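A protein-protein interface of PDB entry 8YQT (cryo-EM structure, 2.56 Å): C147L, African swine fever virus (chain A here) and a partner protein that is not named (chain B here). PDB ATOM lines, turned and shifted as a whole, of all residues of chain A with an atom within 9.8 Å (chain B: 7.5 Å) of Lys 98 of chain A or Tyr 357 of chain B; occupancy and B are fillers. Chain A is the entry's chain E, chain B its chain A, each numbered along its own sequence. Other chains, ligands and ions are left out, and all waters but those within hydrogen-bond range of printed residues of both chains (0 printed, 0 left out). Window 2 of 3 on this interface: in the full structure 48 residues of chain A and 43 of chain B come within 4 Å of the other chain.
Among the printed residues, merely in contact across the chains: Ala 88 of chain A with Thr 353 of chain B, Ala 88 of chain A with Gln 355 of chain B, Ala 88 of chain A with Tyr 357 of chain B, Gly 91 of chain A with Tyr 357 of chain B, Tyr 99 of chain A with Tyr 357 of chain B, Ser 100 of chain A with Asn 358 of chain B and Pro 102 of chain A with Tyr 357 of chain B.
Of the printed residues of chain B, Lys 98 of chain A touches Tyr 357 (2.8 Å).
Tyr 357 of chain B touches just these residues of chain A: Leu 87, Ala 88, Gly 91, Lys 98, Tyr 99, Ser 100 and Pro 102.
Gln 355 of chain B touches just these residues of chain A: Ala 88 (3.8 Å) and Asn 90 (2.9 Å).
His 356 of chain B touches just one residue of chain A: Gly 91.
Of chain A, only Ser 100 comes within 4 Å of Asn 358 of chain B.
Of the printed residues of chain A, Arg 361 of chain B touches Ser 100 (2.8 Å).
Of the printed residues of chain B, Leu 87 of chain A touches Tyr 357.
Printed residues of chain B within 4 Å of Gly 91 of chain A: His 356 and Tyr 357.
Of the printed residues of chain B, Pro 102 of chain A touches Tyr 357 (3.2 Å).
Of the printed residues of chain A, Thr 353 of chain B touches Ala 88 (3.4 Å).
Gln 108 of chain A touches none of the printed residues of chain B.
The nearest residue of chain B that does not touch Lys 98 of chain A is Asn 358 of chain B (4.7 Å).
The nearest printed residue of chain B that does not touch Ala 88 of chain A is Val 354 of chain B (5.6 Å).
The side-chain hydroxyl (OH) of Tyr 357 of chain B sits at hydrogen-bond distance from the backbone carbonyl oxygen (O) of Leu 87 of chain A.
The backbone carbonyl oxygen of Asn 90 of chain A sits at hydrogen-bond distance from the side-chain amide nitrogen of Gln 355 of chain B, at 2.9 Å.
The backbone carbonyl oxygen (O) of Tyr 357 of chain B is in hydrogen-bond range of the side-chain amino group (NZ) of Lys 98 of chain A, 2.8 Å away.
NE of Arg 361 of chain B is in hydrogen-bond range of OG of Ser 100 of chain A (2.8 Å).
The backbone carbonyl oxygen (O) of Tyr 357 of chain B sits close to the side-chain hydroxyl (OG) of Ser 100 of chain A.
A ring nitrogen (NE2) of His 356 of chain B sits at hydrogen-bond distance from the backbone carbonyl oxygen (O) of Gly 91 of chain A, at 3.3 Å.
Of the 12 printed residues of chain B, 6 touch a printed residue of chain A.
Printed residues of chain B that touch a printed residue of chain A: Thr 353, Gln 355, His 356, Tyr 357, Asn 358 and Arg 361.
Hydrophobic or aromatic side chains of chain B that line the printed part of chain A: His 356 and Tyr 357.
Hydrophobic or aromatic side chains of chain A within 4 Å of the printed part of chain B: Pro 102.
Among the printed residues, no Asp or Glu carboxylate lies within 4 Å of a Lys or Arg side-chain nitrogen of the other chain.
NH2 of Arg 361 of chain B is in salt-bridge range of OE1 of Glu 352 of chain B, at 3.2 Å.
ND2 of Asn 358 of chain B lies within hydrogen-bond range of O of Thr 353 of chain B (3.0 Å).
N of Gln 355 of chain B sits at hydrogen-bond distance from OD1 of Asn 358 of chain B, at 2.7 Å.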
ATOM      1  N   ARG A  83      18.727 -20.095  13.264  1.00  0.00           N
ATOM      2  CA  ARG A  83      18.531 -21.533  13.131  1.00  0.00           C
ATOM      3  C   ARG A  83      18.687 -22.253  14.462  1.00  0.00           C
ATOM      4  O   ARG A  83      17.957 -23.212  14.734  1.00  0.00           O
ATOM      5  CB  ARG A  83      19.504 -22.097  12.100  1.00  0.00           C
ATOM      6  CG  ARG A  83      19.344 -23.579  11.862  1.00  0.00           C
ATOM      7  CD  ARG A  83      17.925 -23.902  11.441  1.00  0.00           C
ATOM      8  NE  ARG A  83      17.707 -25.337  11.329  1.00  0.00           N
ATOM      9  CZ  ARG A  83      16.516 -25.906  11.225  1.00  0.00           C
ATOM     10  NH1 ARG A  83      15.408 -25.185  11.209  1.00  0.00           N
ATOM     11  NH2 ARG A  83      16.433 -27.228  11.134  1.00  0.00           N
ATOM     12  N   ALA A  84      19.628 -21.817  15.301  1.00  0.00           N
ATOM     13  CA  ALA A  84      19.777 -22.406  16.623  1.00  0.00           C
ATOM     14  C   ALA A  84      18.547 -22.166  17.482  1.00  0.00           C
ATOM     15  O   ALA A  84      18.130 -23.060  18.225  1.00  0.00           O
ATOM     16  CB  ALA A  84      21.022 -21.846  17.304  1.00  0.00           C
ATOM     17  N   GLN A  85      17.949 -20.977  17.395  1.00  0.00           N
ATOM     18  CA  GLN A  85      16.698 -20.746  18.110  1.00  0.00           C
ATOM     19  C   GLN A  85      15.562 -21.611  17.563  1.00  0.00           C
ATOM     20  O   GLN A  85      14.753 -22.131  18.342  1.00  0.00           O
ATOM     21  CB  GLN A  85      16.332 -19.265  18.054  1.00  0.00           C
ATOM     22  CG  GLN A  85      15.156 -18.890  18.923  1.00  0.00           C
ATOM     23  CD  GLN A  85      15.433 -19.093  20.392  1.00  0.00           C
ATOM     24  OE1 GLN A  85      16.510 -18.769  20.880  1.00  0.00           O
ATOM     25  NE2 GLN A  85      14.457 -19.634  21.107  1.00  0.00           N
ATOM     26  N   GLN A  86      15.484 -21.782  16.240  1.00  0.00           N
ATOM     27  CA  GLN A  86      14.472 -22.677  15.678  1.00  0.00           C
ATOM     28  C   GLN A  86      14.646 -24.093  16.205  1.00  0.00           C
ATOM     29  O   GLN A  86      13.666 -24.756  16.561  1.00  0.00           O
ATOM     30  CB  GLN A  86      14.528 -22.705  14.148  1.00  0.00           C
ATOM     31  CG  GLN A  86      14.770 -21.397  13.447  1.00  0.00           C
ATOM     32  CD  GLN A  86      13.513 -20.609  13.216  1.00  0.00           C
ATOM     33  OE1 GLN A  86      12.725 -20.400  14.130  1.00  0.00           O
ATOM     34  NE2 GLN A  86      13.317 -20.159  11.986  1.00  0.00           N
ATOM     35  N   LEU A  87      15.887 -24.578  16.243  1.00  0.00           N
ATOM     36  CA  LEU A  87      16.149 -25.916  16.758  1.00  0.00           C
ATOM     37  C   LEU A  87      15.819 -26.017  18.237  1.00  0.00           C
ATOM     38  O   LEU A  87      15.350 -27.064  18.695  1.00  0.00           O
ATOM     39  CB  LEU A  87      17.604 -26.299  16.504  1.00  0.00           C
ATOM     40  CG  LEU A  87      17.964 -26.456  15.030  1.00  0.00           C
ATOM     41  CD1 LEU A  87      19.464 -26.418  14.845  1.00  0.00           C
ATOM     42  CD2 LEU A  87      17.386 -27.744  14.478  1.00  0.00           C
ATOM     43  N   ALA A  88      16.060 -24.952  18.998  1.00  0.00           N
ATOM     44  CA  ALA A  88      15.588 -24.908  20.373  1.00  0.00           C
ATOM     45  C   ALA A  88      14.067 -24.941  20.454  1.00  0.00           C
ATOM     46  O   ALA A  88      13.523 -25.332  21.491  1.00  0.00           O
ATOM     47  CB  ALA A  88      16.125 -23.663  21.077  1.00  0.00           C
ATOM     48  N   ILE A  89      13.373 -24.534  19.390  1.00  0.00           N
ATOM     49  CA  ILE A  89      11.915 -24.640  19.369  1.00  0.00           C
ATOM     50  C   ILE A  89      11.475 -26.044  18.965  1.00  0.00           C
ATOM     51  O   ILE A  89      10.687 -26.686  19.668  1.00  0.00           O
ATOM     52  CB  ILE A  89      11.311 -23.571  18.439  1.00  0.00           C
ATOM     53  CG1 ILE A  89      11.475 -22.176  19.044  1.00  0.00           C
ATOM     54  CG2 ILE A  89       9.847 -23.865  18.167  1.00  0.00           C
ATOM     55  CD1 ILE A  89      11.175 -21.054  18.073  1.00  0.00           C
ATOM     56  N   ASN A  90      11.968 -26.545  17.831  1.00  0.00           N
ATOM     57  CA  ASN A  90      11.563 -27.851  17.314  1.00  0.00           C
ATOM     58  C   ASN A  90      12.570 -28.956  17.615  1.00  0.00           C
ATOM     59  O   ASN A  90      12.235 -29.943  18.276  1.00  0.00           O
ATOM     60  CB  ASN A  90      11.336 -27.779  15.799  1.00  0.00           C
ATOM     61  CG  ASN A  90       9.882 -27.631  15.434  1.00  0.00           C
ATOM     62  OD1 ASN A  90       9.000 -28.100  16.152  1.00  0.00           O
ATOM     63  ND2 ASN A  90       9.619 -27.003  14.297  1.00  0.00           N
ATOM     64  N   GLY A  91      13.803 -28.809  17.141  1.00  0.00           N
ATOM     65  CA  GLY A  91      14.770 -29.884  17.185  1.00  0.00           C
ATOM     66  C   GLY A  91      14.790 -30.772  15.960  1.00  0.00           C
ATOM     67  O   GLY A  91      15.552 -31.745  15.936  1.00  0.00           O
ATOM     68  N   SER A  92      13.985 -30.468  14.945  1.00  0.00           N
ATOM     69  CA  SER A  92      13.912 -31.270  13.728  1.00  0.00           C
ATOM     70  C   SER A  92      14.980 -30.790  12.753  1.00  0.00           C
ATOM     71  O   SER A  92      14.903 -29.669  12.239  1.00  0.00           O
ATOM     72  CB  SER A  92      12.523 -31.172  13.106  1.00  0.00           C
ATOM     73  OG  SER A  92      12.491 -31.785  11.830  1.00  0.00           O
ATOM     74  N   THR A  93      15.969 -31.640  12.488  1.00  0.00           N
ATOM     75  CA  THR A  93      17.069 -31.304  11.598  1.00  0.00           C
ATOM     76  C   THR A  93      17.358 -32.470  10.664  1.00  0.00           C
ATOM     77  O   THR A  93      17.070 -33.629  10.971  1.00  0.00           O
ATOM     78  CB  THR A  93      18.341 -30.950  12.378  1.00  0.00           C
ATOM     79  OG1 THR A  93      19.463 -30.965  11.489  1.00  0.00           O
ATOM     80  CG2 THR A  93      18.581 -31.953  13.493  1.00  0.00           C
ATOM     81  N   MET A  94      17.939 -32.144   9.509  1.00  0.00           N
ATOM     82  CA  MET A  94      18.402 -33.142   8.556  1.00  0.00           C
ATOM     83  C   MET A  94      19.894 -33.419   8.680  1.00  0.00           C
ATOM     84  O   MET A  94      20.447 -34.152   7.855  1.00  0.00           O
ATOM     85  CB  MET A  94      18.073 -32.711   7.129  1.00  0.00           C
ATOM     86  CG  MET A  94      18.948 -31.593   6.600  1.00  0.00           C
ATOM     87  SD  MET A  94      18.442 -31.055   4.959  1.00  0.00           S
ATOM     88  CE  MET A  94      17.528 -32.496   4.413  1.00  0.00           C
ATOM     89  N   LEU A  95      20.553 -32.847   9.680  1.00  0.00           N
ATOM     90  CA  LEU A  95      21.957 -33.129   9.932  1.00  0.00           C
ATOM     91  C   LEU A  95      22.134 -34.581  10.358  1.00  0.00           C
ATOM     92  O   LEU A  95      21.296 -35.151  11.064  1.00  0.00           O
ATOM     93  CB  LEU A  95      22.499 -32.193  11.010  1.00  0.00           C
ATOM     94  CG  LEU A  95      23.984 -31.846  10.984  1.00  0.00           C
ATOM     95  CD1 LEU A  95      24.320 -31.000   9.769  1.00  0.00           C
ATOM     96  CD2 LEU A  95      24.354 -31.123  12.258  1.00  0.00           C
ATOM     97  N   LYS A  96      23.240 -35.181   9.923  1.00  0.00           N
ATOM     98  CA  LYS A  96      23.487 -36.596  10.170  1.00  0.00           C
ATOM     99  C   LYS A  96      24.135 -36.845  11.527  1.00  0.00           C
ATOM    100  O   LYS A  96      23.629 -37.644  12.320  1.00  0.00           O
ATOM    101  CB  LYS A  96      24.358 -37.177   9.053  1.00  0.00           C
ATOM    102  CG  LYS A  96      23.674 -37.201   7.698  1.00  0.00           C
ATOM    103  CD  LYS A  96      24.528 -37.896   6.658  1.00  0.00           C
ATOM    104  CE  LYS A  96      23.847 -37.885   5.303  1.00  0.00           C
ATOM    105  NZ  LYS A  96      22.599 -38.691   5.310  1.00  0.00           N
ATOM    106  N   LYS A  97      25.249 -36.175  11.807  1.00  0.00           N
ATOM    107  CA  LYS A  97      25.947 -36.385  13.066  1.00  0.00           C
ATOM    108  C   LYS A  97      25.132 -35.842  14.236  1.00  0.00           C
ATOM    109  O   LYS A  97      24.329 -34.918  14.089  1.00  0.00           O
ATOM    110  CB  LYS A  97      27.321 -35.718  13.033  1.00  0.00           C
ATOM    111  CG  LYS A  97      28.277 -36.316  12.018  1.00  0.00           C
ATOM    112  CD  LYS A  97      29.645 -35.665  12.102  1.00  0.00           C
ATOM    113  CE  LYS A  97      30.745 -36.703  12.241  1.00  0.00           C
ATOM    114  NZ  LYS A  97      31.631 -36.423  13.404  1.00  0.00           N
ATOM    115  N   LYS A  98      25.346 -36.434  15.405  1.00  0.00           N
ATOM    116  CA  LYS A  98      24.655 -36.002  16.612  1.00  0.00           C
ATOM    117  C   LYS A  98      25.442 -34.910  17.319  1.00  0.00           C
ATOM    118  O   LYS A  98      26.665 -34.996  17.465  1.00  0.00           O
ATOM    119  CB  LYS A  98      24.441 -37.184  17.559  1.00  0.00           C
ATOM    120  CG  LYS A  98      23.533 -36.889  18.748  1.00  0.00           C
ATOM    121  CD  LYS A  98      24.334 -36.510  19.994  1.00  0.00           C
ATOM    122  CE  LYS A  98      23.463 -36.487  21.239  1.00  0.00           C
ATOM    123  NZ  LYS A  98      22.354 -35.502  21.144  1.00  0.00           N
ATOM    124  N   TYR A  99      24.729 -33.877  17.761  1.00  0.00           N
ATOM    125  CA  TYR A  99      25.307 -32.814  18.567  1.00  0.00           C
ATOM    126  C   TYR A  99      24.363 -32.515  19.720  1.00  0.00           C
ATOM    127  O   TYR A  99      23.142 -32.589  19.567  1.00  0.00           O
ATOM    128  CB  TYR A  99      25.569 -31.554  17.735  1.00  0.00           C
ATOM    129  CG  TYR A  99      26.551 -31.782  16.612  1.00  0.00           C
ATOM    130  CD1 TYR A  99      26.120 -32.175  15.354  1.00  0.00           C
ATOM    131  CD2 TYR A  99      27.914 -31.620  16.814  1.00  0.00           C
ATOM    132  CE1 TYR A  99      27.016 -32.392  14.329  1.00  0.00           C
ATOM    133  CE2 TYR A  99      28.816 -31.833  15.797  1.00  0.00           C
ATOM    134  CZ  TYR A  99      28.362 -32.220  14.556  1.00  0.00           C
ATOM    135  OH  TYR A  99      29.260 -32.435  13.539  1.00  0.00           O
ATOM    136  N   SER A 100      24.934 -32.178  20.870  1.00  0.00           N
ATOM    137  CA  SER A 100      24.174 -32.026  22.100  1.00  0.00           C
ATOM    138  C   SER A 100      23.715 -30.596  22.354  1.00  0.00           C
ATOM    139  O   SER A 100      23.123 -30.330  23.403  1.00  0.00           O
ATOM    140  CB  SER A 100      25.000 -32.521  23.288  1.00  0.00           C
ATOM    141  OG  SER A 100      24.319 -32.292  24.507  1.00  0.00           O
ATOM    142  N   SER A 101      23.980 -29.673  21.439  1.00  0.00           N
ATOM    143  CA  SER A 101      23.562 -28.294  21.617  1.00  0.00           C
ATOM    144  C   SER A 101      23.025 -27.747  20.304  1.00  0.00           C
ATOM    145  O   SER A 101      23.489 -28.139  19.229  1.00  0.00           O
ATOM    146  CB  SER A 101      24.731 -27.429  22.112  1.00  0.00           C
ATOM    147  OG  SER A 101      24.368 -26.067  22.249  1.00  0.00           O
ATOM    148  N   PRO A 102      22.033 -26.852  20.359  1.00  0.00           N
ATOM    149  CA  PRO A 102      21.496 -26.285  19.112  1.00  0.00           C
ATOM    150  C   PRO A 102      22.520 -25.506  18.314  1.00  0.00           C
ATOM    151  O   PRO A 102      22.447 -25.491  17.080  1.00  0.00           O
ATOM    152  CB  PRO A 102      20.359 -25.374  19.598  1.00  0.00           C
ATOM    153  CG  PRO A 102      20.069 -25.814  20.991  1.00  0.00           C
ATOM    154  CD  PRO A 102      21.360 -26.302  21.545  1.00  0.00           C
ATOM    155  N   ILE A 103      23.467 -24.849  18.985  1.00  0.00           N
ATOM    156  CA  ILE A 103      24.424 -24.001  18.287  1.00  0.00           C
ATOM    157  C   ILE A 103      25.310 -24.827  17.365  1.00  0.00           C
ATOM    158  O   ILE A 103      25.545 -24.447  16.216  1.00  0.00           O
ATOM    159  CB  ILE A 103      25.250 -23.184  19.295  1.00  0.00           C
ATOM    160  CG1 ILE A 103      24.325 -22.304  20.135  1.00  0.00           C
ATOM    161  CG2 ILE A 103      26.285 -22.351  18.572  1.00  0.00           C
ATOM    162  CD1 ILE A 103      25.008 -21.576  21.258  1.00  0.00           C
ATOM    163  N   ASP A 104      25.813 -25.967  17.844  1.00  0.00           N
ATOM    164  CA  ASP A 104      26.674 -26.797  17.007  1.00  0.00           C
ATOM    165  C   ASP A 104      25.909 -27.387  15.832  1.00  0.00           C
ATOM    166  O   ASP A 104      26.451 -27.497  14.727  1.00  0.00           O
ATOM    167  CB  ASP A 104      27.319 -27.899  17.842  1.00  0.00           C
ATOM    168  CG  ASP A 104      27.735 -27.415  19.206  1.00  0.00           C
ATOM    169  OD1 ASP A 104      28.945 -27.454  19.510  1.00  0.00           O
ATOM    170  OD2 ASP A 104      26.857 -26.972  19.968  1.00  0.00           O
ATOM    171  N   ILE A 105      24.646 -27.760  16.044  1.00  0.00           N
ATOM    172  CA  ILE A 105      23.820 -28.214  14.933  1.00  0.00           C
ATOM    173  C   ILE A 105      23.665 -27.106  13.901  1.00  0.00           C
ATOM    174  O   ILE A 105      23.751 -27.350  12.695  1.00  0.00           O
ATOM    175  CB  ILE A 105      22.454 -28.705  15.440  1.00  0.00           C
ATOM    176  CG1 ILE A 105      22.631 -29.754  16.536  1.00  0.00           C
ATOM    177  CG2 ILE A 105      21.641 -29.276  14.295  1.00  0.00           C
ATOM    178  CD1 ILE A 105      21.390 -29.982  17.357  1.00  0.00           C
ATOM    179  N   ALA A 106      23.436 -25.871  14.355  1.00  0.00           N
ATOM    180  CA  ALA A 106      23.272 -24.759  13.424  1.00  0.00           C
ATOM    181  C   ALA A 106      24.550 -24.488  12.636  1.00  0.00           C
ATOM    182  O   ALA A 106      24.501 -24.294  11.415  1.00  0.00           O
ATOM    183  CB  ALA A 106      22.831 -23.510  14.181  1.00  0.00           C
ATOM    184  N   GLN A 108      27.016 -26.603  12.012  1.00  0.00           N
ATOM    185  CA  GLN A 108      27.276 -27.705  11.095  1.00  0.00           C
ATOM    186  C   GLN A 108      26.314 -27.693   9.917  1.00  0.00           C
ATOM    187  O   GLN A 108      26.700 -28.054   8.802  1.00  0.00           O
ATOM    188  CB  GLN A 108      27.205 -29.036  11.836  1.00  0.00           C
ATOM    189  CG  GLN A 108      28.543 -29.729  11.970  1.00  0.00           C
ATOM    190  CD  GLN A 108      29.632 -28.800  12.456  1.00  0.00           C
ATOM    191  OE1 GLN A 108      29.564 -28.273  13.564  1.00  0.00           O
ATOM    192  NE2 GLN A 108      30.644 -28.592  11.624  1.00  0.00           N
ATOM    193  N   GLU B 352      18.991 -23.116  29.255  1.00  0.00           N
ATOM    194  CA  GLU B 352      19.073 -24.307  28.418  1.00  0.00           C
ATOM    195  C   GLU B 352      17.667 -24.826  28.164  1.00  0.00           C
ATOM    196  O   GLU B 352      16.938 -25.138  29.110  1.00  0.00           O
ATOM    197  CB  GLU B 352      19.926 -25.387  29.084  1.00  0.00           C
ATOM    198  CG  GLU B 352      21.398 -25.048  29.198  1.00  0.00           C
ATOM    199  CD  GLU B 352      22.130 -25.179  27.880  1.00  0.00           C
ATOM    200  OE1 GLU B 352      21.698 -25.992  27.036  1.00  0.00           O
ATOM    201  OE2 GLU B 352      23.141 -24.478  27.690  1.00  0.00           O
ATOM    202  N   THR B 353      17.291 -24.926  26.892  1.00  0.00           N
ATOM    203  CA  THR B 353      15.975 -25.427  26.515  1.00  0.00           C
ATOM    204  C   THR B 353      16.058 -26.934  26.315  1.00  0.00           C
ATOM    205  O   THR B 353      16.854 -27.416  25.502  1.00  0.00           O
ATOM    206  CB  THR B 353      15.466 -24.741  25.249  1.00  0.00           C
ATOM    207  OG1 THR B 353      15.364 -23.331  25.480  1.00  0.00           O
ATOM    208  CG2 THR B 353      14.100 -25.277  24.869  1.00  0.00           C
ATOM    209  N   VAL B 354      15.234 -27.674  27.054  1.00  0.00           N
ATOM    210  CA  VAL B 354      15.315 -29.130  27.056  1.00  0.00           C
ATOM    211  C   VAL B 354      14.774 -29.666  25.738  1.00  0.00           C
ATOM    212  O   VAL B 354      13.645 -29.358  25.340  1.00  0.00           O
ATOM    213  CB  VAL B 354      14.552 -29.717  28.251  1.00  0.00           C
ATOM    214  CG1 VAL B 354      14.648 -31.229  28.248  1.00  0.00           C
ATOM    215  CG2 VAL B 354      15.083 -29.147  29.553  1.00  0.00           C
ATOM    216  N   GLN B 355      15.582 -30.469  25.053  1.00  0.00           N
ATOM    217  CA  GLN B 355      15.178 -31.112  23.812  1.00  0.00           C
ATOM    218  C   GLN B 355      15.663 -32.555  23.852  1.00  0.00           C
ATOM    219  O   GLN B 355      16.203 -33.022  24.857  1.00  0.00           O
ATOM    220  CB  GLN B 355      15.720 -30.353  22.594  1.00  0.00           C
ATOM    221  CG  GLN B 355      14.938 -29.106  22.233  1.00  0.00           C
ATOM    222  CD  GLN B 355      13.489 -29.398  21.910  1.00  0.00           C
ATOM    223  OE1 GLN B 355      12.581 -28.833  22.516  1.00  0.00           O
ATOM    224  NE2 GLN B 355      13.264 -30.290  20.955  1.00  0.00           N
ATOM    225  N   HIS B 356      15.467 -33.270  22.744  1.00  0.00           N
ATOM    226  CA  HIS B 356      15.884 -34.665  22.691  1.00  0.00           C
ATOM    227  C   HIS B 356      17.398 -34.802  22.598  1.00  0.00           C
ATOM    228  O   HIS B 356      17.953 -35.816  23.034  1.00  0.00           O
ATOM    229  CB  HIS B 356      15.216 -35.371  21.511  1.00  0.00           C
ATOM    230  CG  HIS B 356      15.716 -34.916  20.175  1.00  0.00           C
ATOM    231  ND1 HIS B 356      16.409 -35.743  19.319  1.00  0.00           N
ATOM    232  CD2 HIS B 356      15.615 -33.722  19.545  1.00  0.00           C
ATOM    233  CE1 HIS B 356      16.719 -35.077  18.221  1.00  0.00           C
ATOM    234  NE2 HIS B 356      16.248 -33.848  18.333  1.00  0.00           N
ATOM    235  N   TYR B 357      18.083 -33.807  22.039  1.00  0.00           N
ATOM    236  CA  TYR B 357      19.522 -33.907  21.839  1.00  0.00           C
ATOM    237  C   TYR B 357      20.338 -33.462  23.046  1.00  0.00           C
ATOM    238  O   TYR B 357      21.557 -33.655  23.046  1.00  0.00           O
ATOM    239  CB  TYR B 357      19.949 -33.095  20.608  1.00  0.00           C
ATOM    240  CG  TYR B 357      19.358 -31.707  20.537  1.00  0.00           C
ATOM    241  CD1 TYR B 357      19.890 -30.664  21.281  1.00  0.00           C
ATOM    242  CD2 TYR B 357      18.274 -31.437  19.716  1.00  0.00           C
ATOM    243  CE1 TYR B 357      19.351 -29.397  21.217  1.00  0.00           C
ATOM    244  CE2 TYR B 357      17.731 -30.173  19.644  1.00  0.00           C
ATOM    245  CZ  TYR B 357      18.273 -29.157  20.397  1.00  0.00           C
ATOM    246  OH  TYR B 357      17.734 -27.897  20.328  1.00  0.00           O
ATOM    247  N   ASN B 358      19.708 -32.887  24.078  1.00  0.00           N
ATOM    248  CA  ASN B 358      20.468 -32.441  25.240  1.00  0.00           C
ATOM    249  C   ASN B 358      19.823 -32.848  26.560  1.00  0.00           C
ATOM    250  O   ASN B 358      20.182 -32.300  27.607  1.00  0.00           O
ATOM    251  CB  ASN B 358      20.669 -30.920  25.219  1.00  0.00           C
ATOM    252  CG  ASN B 358      19.363 -30.150  25.181  1.00  0.00           C
ATOM    253  OD1 ASN B 358      18.280 -30.726  25.243  1.00  0.00           O
ATOM    254  ND2 ASN B 358      19.465 -28.832  25.080  1.00  0.00           N
ATOM    255  N   ILE B 359      18.881 -33.791  26.542  1.00  0.00           N
ATOM    256  CA  ILE B 359      18.246 -34.223  27.782  1.00  0.00           C
ATOM    257  C   ILE B 359      19.244 -34.955  28.671  1.00  0.00           C
ATOM    258  O   ILE B 359      19.219 -34.818  29.899  1.00  0.00           O
ATOM    259  CB  ILE B 359      17.006 -35.084  27.470  1.00  0.00           C
ATOM    260  CG1 ILE B 359      16.367 -35.605  28.759  1.00  0.00           C
ATOM    261  CG2 ILE B 359      17.360 -36.224  26.523  1.00  0.00           C
ATOM    262  CD1 ILE B 359      15.775 -34.522  29.625  1.00  0.00           C
ATOM    263  N   ASN B 360      20.144 -35.735  28.070  1.00  0.00           N
ATOM    264  CA  ASN B 360      21.124 -36.480  28.852  1.00  0.00           C
ATOM    265  C   ASN B 360      22.222 -35.582  29.406  1.00  0.00           C
ATOM    266  O   ASN B 360      22.708 -35.821  30.517  1.00  0.00           O
ATOM    267  CB  ASN B 360      21.736 -37.592  28.002  1.00  0.00           C
ATOM    268  CG  ASN B 360      20.750 -38.703  27.703  1.00  0.00           C
ATOM    269  OD1 ASN B 360      20.015 -39.147  28.582  1.00  0.00           O
ATOM    270  ND2 ASN B 360      20.730 -39.155  26.456  1.00  0.00           N
ATOM    271  N   ARG B 361      22.627 -34.560  28.652  1.00  0.00           N
ATOM    272  CA  ARG B 361      23.668 -33.654  29.128  1.00  0.00           C
ATOM    273  C   ARG B 361      23.160 -32.767  30.257  1.00  0.00           C
ATOM    274  O   ARG B 361      23.903 -32.465  31.197  1.00  0.00           O
ATOM    275  CB  ARG B 361      24.190 -32.803  27.970  1.00  0.00           C
ATOM    276  CG  ARG B 361      25.196 -31.746  28.381  1.00  0.00           C
ATOM    277  CD  ARG B 361      25.768 -31.010  27.180  1.00  0.00           C
ATOM    278  NE  ARG B 361      24.740 -30.315  26.412  1.00  0.00           N
ATOM    279  CZ  ARG B 361      24.193 -29.161  26.764  1.00  0.00           C
ATOM    280  NH1 ARG B 361      24.537 -28.544  27.883  1.00  0.00           N
ATOM    281  NH2 ARG B 361      23.276 -28.611  25.973  1.00  0.00           N
ATOM    282  N   LEU B 362      21.902 -32.339  30.184  1.00  0.00           N
ATOM    283  CA  LEU B 362      21.362 -31.397  31.154  1.00  0.00           C
ATOM    284  C   LEU B 362      20.888 -32.059  32.438  1.00  0.00           C
ATOM    285  O   LEU B 362      20.636 -31.353  33.420  1.00  0.00           O
ATOM    286  CB  LEU B 362      20.204 -30.615  30.532  1.00  0.00           C
ATOM    287  CG  LEU B 362      20.588 -29.665  29.402  1.00  0.00           C
ATOM    288  CD1 LEU B 362      19.348 -29.042  28.788  1.00  0.00           C
ATOM    289  CD2 LEU B 362      21.539 -28.602  29.910  1.00  0.00           C
ATOM    290  N   VAL B 401      10.654 -32.075  27.192  1.00  0.00           N
ATOM    291  CA  VAL B 401      11.049 -31.361  25.983  1.00  0.00           C
ATOM    292  C   VAL B 401      10.240 -30.077  25.874  1.00  0.00           C
ATOM    293  O   VAL B 401       9.004 -30.103  25.845  1.00  0.00           O
ATOM    294  CB  VAL B 401      10.867 -32.250  24.749  1.00  0.00           C
ATOM    295  CG1 VAL B 401      10.836 -31.410  23.490  1.00  0.00           C
ATOM    296  CG2 VAL B 401      11.983 -33.278  24.675  1.00  0.00           C
